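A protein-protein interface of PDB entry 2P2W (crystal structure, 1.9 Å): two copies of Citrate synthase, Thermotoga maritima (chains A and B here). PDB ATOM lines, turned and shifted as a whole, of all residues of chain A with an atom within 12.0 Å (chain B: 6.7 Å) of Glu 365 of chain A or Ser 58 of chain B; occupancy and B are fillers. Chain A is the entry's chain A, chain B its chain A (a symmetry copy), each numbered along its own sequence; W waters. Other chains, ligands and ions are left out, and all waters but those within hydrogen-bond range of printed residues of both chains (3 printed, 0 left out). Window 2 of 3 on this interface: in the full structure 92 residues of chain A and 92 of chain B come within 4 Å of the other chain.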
ATOM      1  N   ILE A 358      11.167 -21.450   6.567  1.00  0.00           N
ATOM      2  CA  ILE A 358      10.756 -22.593   7.371  1.00  0.00           C
ATOM      3  C   ILE A 358      10.607 -23.835   6.499  1.00  0.00           C
ATOM      4  O   ILE A 358       9.907 -23.805   5.486  1.00  0.00           O
ATOM      5  CB  ILE A 358       9.403 -22.316   8.067  1.00  0.00           C
ATOM      6  CG1 ILE A 358       9.528 -21.100   8.987  1.00  0.00           C
ATOM      7  CG2 ILE A 358       8.950 -23.544   8.845  1.00  0.00           C
ATOM      8  CD1 ILE A 358       8.838 -21.264  10.322  1.00  0.00           C
ATOM      9  N   PRO A 359      11.281 -24.941   6.865  1.00  0.00           N
ATOM     10  CA  PRO A 359      11.152 -26.155   6.053  1.00  0.00           C
ATOM     11  C   PRO A 359       9.670 -26.502   5.950  1.00  0.00           C
ATOM     12  O   PRO A 359       8.936 -26.423   6.933  1.00  0.00           O
ATOM     13  CB  PRO A 359      11.968 -27.189   6.832  1.00  0.00           C
ATOM     14  CG  PRO A 359      12.893 -26.440   7.754  1.00  0.00           C
ATOM     15  CD  PRO A 359      12.128 -25.183   8.045  1.00  0.00           C
ATOM     16  N   ILE A 360       9.240 -26.876   4.751  1.00  0.00           N
ATOM     17  CA  ILE A 360       7.837 -27.166   4.490  1.00  0.00           C
ATOM     18  C   ILE A 360       7.107 -28.044   5.511  1.00  0.00           C
ATOM     19  O   ILE A 360       5.935 -27.805   5.798  1.00  0.00           O
ATOM     20  CB  ILE A 360       7.668 -27.748   3.059  1.00  0.00           C
ATOM     21  CG1 ILE A 360       6.214 -27.612   2.613  1.00  0.00           C
ATOM     22  CG2 ILE A 360       8.129 -29.195   3.013  1.00  0.00           C
ATOM     23  CD1 ILE A 360       6.039 -27.649   1.112  1.00  0.00           C
ATOM     24  N   GLU A 361       7.787 -29.038   6.074  1.00  0.00           N
ATOM     25  CA  GLU A 361       7.145 -29.914   7.055  1.00  0.00           C
ATOM     26  C   GLU A 361       6.802 -29.245   8.387  1.00  0.00           C
ATOM     27  O   GLU A 361       6.026 -29.793   9.172  1.00  0.00           O
ATOM     28  CB  GLU A 361       8.007 -31.156   7.323  1.00  0.00           C
ATOM     29  CG  GLU A 361       9.501 -30.924   7.237  1.00  0.00           C
ATOM     30  CD  GLU A 361      10.004 -30.967   5.808  1.00  0.00           C
ATOM     31  OE1 GLU A 361       9.840 -32.020   5.152  1.00  0.00           O
ATOM     32  OE2 GLU A 361      10.556 -29.953   5.338  1.00  0.00           O
ATOM     33  N   ARG A 362       7.363 -28.065   8.642  1.00  0.00           N
ATOM     34  CA  ARG A 362       7.100 -27.357   9.893  1.00  0.00           C
ATOM     35  C   ARG A 362       6.191 -26.147   9.722  1.00  0.00           C
ATOM     36  O   ARG A 362       5.990 -25.388  10.667  1.00  0.00           O
ATOM     37  CB  ARG A 362       8.405 -26.865  10.523  1.00  0.00           C
ATOM     38  CG  ARG A 362       9.485 -27.906  10.716  1.00  0.00           C
ATOM     39  CD  ARG A 362      10.712 -27.235  11.311  1.00  0.00           C
ATOM     40  NE  ARG A 362      11.928 -28.021  11.139  1.00  0.00           N
ATOM     41  CZ  ARG A 362      13.155 -27.516  11.228  1.00  0.00           C
ATOM     42  NH1 ARG A 362      13.322 -26.225  11.486  1.00  0.00           N
ATOM     43  NH2 ARG A 362      14.213 -28.298  11.058  1.00  0.00           N
ATOM     44  N   ARG A 363       5.642 -25.962   8.528  1.00  0.00           N
ATOM     45  CA  ARG A 363       4.786 -24.811   8.268  1.00  0.00           C
ATOM     46  C   ARG A 363       3.371 -24.925   8.822  1.00  0.00           C
ATOM     47  O   ARG A 363       2.750 -25.987   8.773  1.00  0.00           O
ATOM     48  CB  ARG A 363       4.755 -24.532   6.764  1.00  0.00           C
ATOM     49  CG  ARG A 363       6.133 -24.177   6.230  1.00  0.00           C
ATOM     50  CD  ARG A 363       6.174 -24.038   4.724  1.00  0.00           C
ATOM     51  NE  ARG A 363       7.545 -23.835   4.271  1.00  0.00           N
ATOM     52  CZ  ARG A 363       7.943 -23.940   3.009  1.00  0.00           C
ATOM     53  NH1 ARG A 363       7.070 -24.242   2.056  1.00  0.00           N
ATOM     54  NH2 ARG A 363       9.218 -23.746   2.701  1.00  0.00           N
ATOM     55  N   ASP A 364       2.874 -23.809   9.354  1.00  0.00           N
ATOM     56  CA  ASP A 364       1.534 -23.739   9.936  1.00  0.00           C
ATOM     57  C   ASP A 364       0.473 -24.228   8.951  1.00  0.00           C
ATOM     58  O   ASP A 364       0.250 -23.606   7.905  1.00  0.00           O
ATOM     59  CB  ASP A 364       1.228 -22.293  10.341  1.00  0.00           C
ATOM     60  CG  ASP A 364      -0.075 -22.161  11.098  1.00  0.00           C
ATOM     61  OD1 ASP A 364      -0.622 -23.197  11.548  1.00  0.00           O
ATOM     62  OD2 ASP A 364      -0.557 -21.014  11.249  1.00  0.00           O
ATOM     63  N   GLU A 365      -0.188 -25.331   9.290  1.00  0.00           N
ATOM     64  CA  GLU A 365      -1.226 -25.902   8.436  1.00  0.00           C
ATOM     65  C   GLU A 365      -2.511 -25.092   8.561  1.00  0.00           C
ATOM     66  O   GLU A 365      -2.623 -24.308   9.530  1.00  0.00           O
ATOM     67  CB  GLU A 365      -1.489 -27.358   8.839  1.00  0.00           C
ATOM     68  CG  GLU A 365      -2.460 -28.084   7.914  1.00  0.00           C
ATOM     69  CD  GLU A 365      -1.878 -28.301   6.530  1.00  0.00           C
ATOM     70  OE1 GLU A 365      -0.644 -28.494   6.431  1.00  0.00           O
ATOM     71  OE2 GLU A 365      -2.651 -28.289   5.543  1.00  0.00           O
ATOM     72  N   PRO B  55       4.066 -21.897   0.981  1.00  0.00           N
ATOM     73  CA  PRO B  55       2.987 -22.885   0.885  1.00  0.00           C
ATOM     74  C   PRO B  55       3.200 -24.133   1.734  1.00  0.00           C
ATOM     75  O   PRO B  55       4.335 -24.557   1.959  1.00  0.00           O
ATOM     76  CB  PRO B  55       2.970 -23.220  -0.598  1.00  0.00           C
ATOM     77  CG  PRO B  55       4.438 -23.200  -0.929  1.00  0.00           C
ATOM     78  CD  PRO B  55       4.912 -21.930  -0.227  1.00  0.00           C
ATOM     79  N   THR B  56       2.098 -24.714   2.205  1.00  0.00           N
ATOM     80  CA  THR B  56       2.170 -25.944   2.980  1.00  0.00           C
ATOM     81  C   THR B  56       2.400 -27.050   1.955  1.00  0.00           C
ATOM     82  O   THR B  56       2.353 -26.802   0.748  1.00  0.00           O
ATOM     83  CB  THR B  56       0.852 -26.239   3.732  1.00  0.00           C
ATOM     84  OG1 THR B  56      -0.225 -26.325   2.791  1.00  0.00           O
ATOM     85  CG2 THR B  56       0.558 -25.148   4.753  1.00  0.00           C
ATOM     86  N   LYS B  57       2.641 -28.265   2.430  1.00  0.00           N
ATOM     87  CA  LYS B  57       2.884 -29.392   1.538  1.00  0.00           C
ATOM     88  C   LYS B  57       1.774 -29.562   0.501  1.00  0.00           C
ATOM     89  O   LYS B  57       2.046 -29.709  -0.692  1.00  0.00           O
ATOM     90  CB  LYS B  57       3.034 -30.686   2.347  1.00  0.00           C
ATOM     91  CG  LYS B  57       3.359 -31.909   1.497  1.00  0.00           C
ATOM     92  CD  LYS B  57       3.455 -33.174   2.341  1.00  0.00           C
ATOM     93  CE  LYS B  57       3.657 -34.405   1.468  1.00  0.00           C
ATOM     94  NZ  LYS B  57       3.694 -35.659   2.274  1.00  0.00           N
ATOM     95  N   SER B  58       0.522 -29.544   0.952  1.00  0.00           N
ATOM     96  CA  SER B  58      -0.604 -29.707   0.037  1.00  0.00           C
ATOM     97  C   SER B  58      -0.775 -28.506  -0.894  1.00  0.00           C
ATOM     98  O   SER B  58      -1.106 -28.668  -2.068  1.00  0.00           O
ATOM     99  CB  SER B  58      -1.902 -29.957   0.819  1.00  0.00           C
ATOM    100  OG  SER B  58      -2.191 -28.890   1.704  1.00  0.00           O
ATOM    101  N   GLU B  59      -0.553 -27.304  -0.377  1.00  0.00           N
ATOM    102  CA  GLU B  59      -0.680 -26.114  -1.210  1.00  0.00           C
ATOM    103  C   GLU B  59       0.346 -26.143  -2.342  1.00  0.00           C
ATOM    104  O   GLU B  59       0.012 -25.873  -3.496  1.00  0.00           O
ATOM    105  CB  GLU B  59      -0.510 -24.843  -0.371  1.00  0.00           C
ATOM    106  CG  GLU B  59      -1.812 -24.350   0.253  1.00  0.00           C
ATOM    107  CD  GLU B  59      -1.585 -23.382   1.394  1.00  0.00           C
ATOM    108  OE1 GLU B  59      -0.452 -23.332   1.916  1.00  0.00           O
ATOM    109  OE2 GLU B  59      -2.543 -22.675   1.779  1.00  0.00           O
ATOM    110  N   LEU B  60       1.591 -26.481  -2.017  1.00  0.00           N
ATOM    111  CA  LEU B  60       2.635 -26.542  -3.035  1.00  0.00           C
ATOM    112  C   LEU B  60       2.321 -27.619  -4.066  1.00  0.00           C
ATOM    113  O   LEU B  60       2.498 -27.414  -5.266  1.00  0.00           O
ATOM    114  CB  LEU B  60       3.995 -26.835  -2.397  1.00  0.00           C
ATOM    115  CG  LEU B  60       5.168 -26.883  -3.384  1.00  0.00           C
ATOM    116  CD1 LEU B  60       5.251 -25.568  -4.142  1.00  0.00           C
ATOM    117  CD2 LEU B  60       6.463 -27.143  -2.633  1.00  0.00           C
ATOM    118  N   GLU B  61       1.855 -28.769  -3.589  1.00  0.00           N
ATOM    119  CA  GLU B  61       1.513 -29.879  -4.468  1.00  0.00           C
ATOM    120  C   GLU B  61       0.439 -29.450  -5.463  1.00  0.00           C
ATOM    121  O   GLU B  61       0.558 -29.687  -6.665  1.00  0.00           O
ATOM    122  CB  GLU B  61       1.008 -31.068  -3.646  1.00  0.00           C
ATOM    123  CG  GLU B  61       0.924 -32.368  -4.428  1.00  0.00           C
ATOM    124  CD  GLU B  61       0.217 -33.478  -3.660  1.00  0.00           C
ATOM    125  OE1 GLU B  61      -0.949 -33.279  -3.248  1.00  0.00           O
ATOM    126  OE2 GLU B  61       0.832 -34.550  -3.471  1.00  0.00           O
ATOM    127  N   GLU B  62      -0.614 -28.820  -4.951  1.00  0.00           N
ATOM    128  CA  GLU B  62      -1.709 -28.356  -5.795  1.00  0.00           C
ATOM    129  C   GLU B  62      -1.264 -27.231  -6.727  1.00  0.00           C
ATOM    130  O   GLU B  62      -1.690 -27.162  -7.881  1.00  0.00           O
ATOM    131  CB  GLU B  62      -2.875 -27.885  -4.922  1.00  0.00           C
ATOM    132  CG  GLU B  62      -3.655 -29.026  -4.289  1.00  0.00           C
ATOM    133  CD  GLU B  62      -4.475 -28.583  -3.092  1.00  0.00           C
ATOM    134  OE1 GLU B  62      -4.965 -27.432  -3.096  1.00  0.00           O
ATOM    135  OE2 GLU B  62      -4.637 -29.392  -2.152  1.00  0.00           O
ATOM    136  N   PHE B  63      -0.400 -26.352  -6.230  1.00  0.00           N
ATOM    137  CA  PHE B  63       0.084 -25.248  -7.046  1.00  0.00           C
ATOM    138  C   PHE B  63       0.967 -25.773  -8.179  1.00  0.00           C
ATOM    139  O   PHE B  63       0.938 -25.245  -9.290  1.00  0.00           O
ATOM    140  CB  PHE B  63       0.869 -24.248  -6.189  1.00  0.00           C
ATOM    141  CG  PHE B  63       1.275 -23.000  -6.929  1.00  0.00           C
ATOM    142  CD1 PHE B  63       0.310 -22.117  -7.415  1.00  0.00           C
ATOM    143  CD2 PHE B  63       2.618 -22.717  -7.156  1.00  0.00           C
ATOM    144  CE1 PHE B  63       0.678 -20.967  -8.122  1.00  0.00           C
ATOM    145  CE2 PHE B  63       2.999 -21.571  -7.861  1.00  0.00           C
ATOM    146  CZ  PHE B  63       2.027 -20.695  -8.345  1.00  0.00           C
ATOM    147  N   ARG B  65       0.692 -28.674  -9.633  1.00  0.00           N
ATOM    148  CA  ARG B  65      -0.182 -29.303 -10.619  1.00  0.00           C
ATOM    149  C   ARG B  65      -0.894 -28.239 -11.452  1.00  0.00           C
ATOM    150  O   ARG B  65      -1.166 -28.447 -12.635  1.00  0.00           O
ATOM    151  CB  ARG B  65      -1.215 -30.208  -9.936  1.00  0.00           C
ATOM    152  CG  ARG B  65      -0.625 -31.475  -9.328  1.00  0.00           C
ATOM    153  CD  ARG B  65      -1.677 -32.573  -9.248  1.00  0.00           C
ATOM    154  NE  ARG B  65      -2.816 -32.188  -8.425  1.00  0.00           N
ATOM    155  CZ  ARG B  65      -2.939 -32.481  -7.133  1.00  0.00           C
ATOM    156  NH1 ARG B  65      -1.989 -33.168  -6.513  1.00  0.00           N
ATOM    157  NH2 ARG B  65      -4.008 -32.080  -6.461  1.00  0.00           N
HETATM  158  O   HOH W   1      -2.799 -26.340   3.633  1.00  0.00           O
HETATM  159  O   HOH W   2      -0.254 -29.715   3.869  1.00  0.00           O
HETATM  160  O   HOH W   3       3.351 -28.633   5.141  1.00  0.00           O
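The backbone carbonyl oxygen (O) of Pro 55 of chain B sits at hydrogen-bond distance from the guanidinium group (NH1) of Arg 363 of chain A, 2.8 Å away.
N of Thr 56 of chain B is in hydrogen-bond range of OE1 of Glu 59 of chain B (2.9 Å).
The backbone carbonyl oxygen (O) of Ile 358 of chain A sits at hydrogen-bond distance from the guanidinium group (NE) of Arg 363 of chain A (2.7 Å).
The side-chain hydroxyl (OG) of Ser 58 of chain B sits at hydrogen-bond distance from the side-chain hydroxyl (OG1) of Thr 56 of chain B, at 3.4 Å.
Ile 360 of chain A touches Pro 55 of chain B.
Ile 360 of chain A touches Thr 56 of chain B.
Lys 57 of chain B touches Ile 360 of chain A.
Ile 360 of chain A touches Leu 60 of chain B.
Thr 56 of chain B touches Asp 364 of chain A (CG2 to O, 3.5 Å).
Thr 56 of chain B touches Glu 365 of chain A.
Glu 365 of chain A touches Ser 58 of chain B.
Arg 362 of chain A touches none of the printed residues of chain B.
Printed residues of chain B within 4 Å of Arg 363 of chain A: Pro 55 (2.8 Å).
Of the printed residues of chain B, Asp 364 of chain A touches Thr 56.
Glu 365 of chain A touches just these residues of chain B: Thr 56 (3.8 Å) and Ser 58 (3.9 Å).
Printed residues of chain A within 4 Å of Pro 55 of chain B: Ile 360 (3.6 Å) and Arg 363 (2.8 Å).
Of chain A, only Ile 360 (3.6 Å) comes within 4 Å of Lys 57 of chain B.
Ser 58 of chain B touches just one residue of chain A: Glu 365.
No residue of chain A comes within 4 Å of Glu 59 of chain B.
No residue of chain A comes within 4 Å of Glu 61 of chain B.
No residue of chain A comes within 4 Å of Glu 62 of chain B.
The nearest residue of chain B that does not touch Glu 365 of chain A is Lys 57 of chain B (5.2 Å).
Of the 10 printed residues of chain B, 5 touch a printed residue of chain A.
Hydrophobic or aromatic side chains of chain B that line the printed part of chain A: Pro 55 and Leu 60.
Of the 8 printed residues of chain A, 4 touch a printed residue of chain B.
Hydrophobic or aromatic side chains of chain A that line the printed part of chain B: Ile 360.
Among the printed residues, no Asp or Glu carboxylate lies within 4 Å of a Lys or Arg side-chain nitrogen of the other chain.
No position is printed for both chains.
Of the 8 pairs that touch across the chains among the printed residues, none has its exchanged pair printed and touching as well.
Water W1 lies within hydrogen-bond range of OG1 of Thr 56 of chain B (2.7 Å), OE2 of Glu 365 of chain A (2.7 Å) and OG of Ser 58 of chain B (3.3 Å).
Water W3 lies within hydrogen-bond range of O of Ile 360 of chain A (2.8 Å) and N of Lys 57 of chain B (2.8 Å).
Water W2 lies within hydrogen-bond range of OE1 of Glu 365 of chain A (2.9 Å) and OG of Ser 58 of chain B (3.0 Å).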
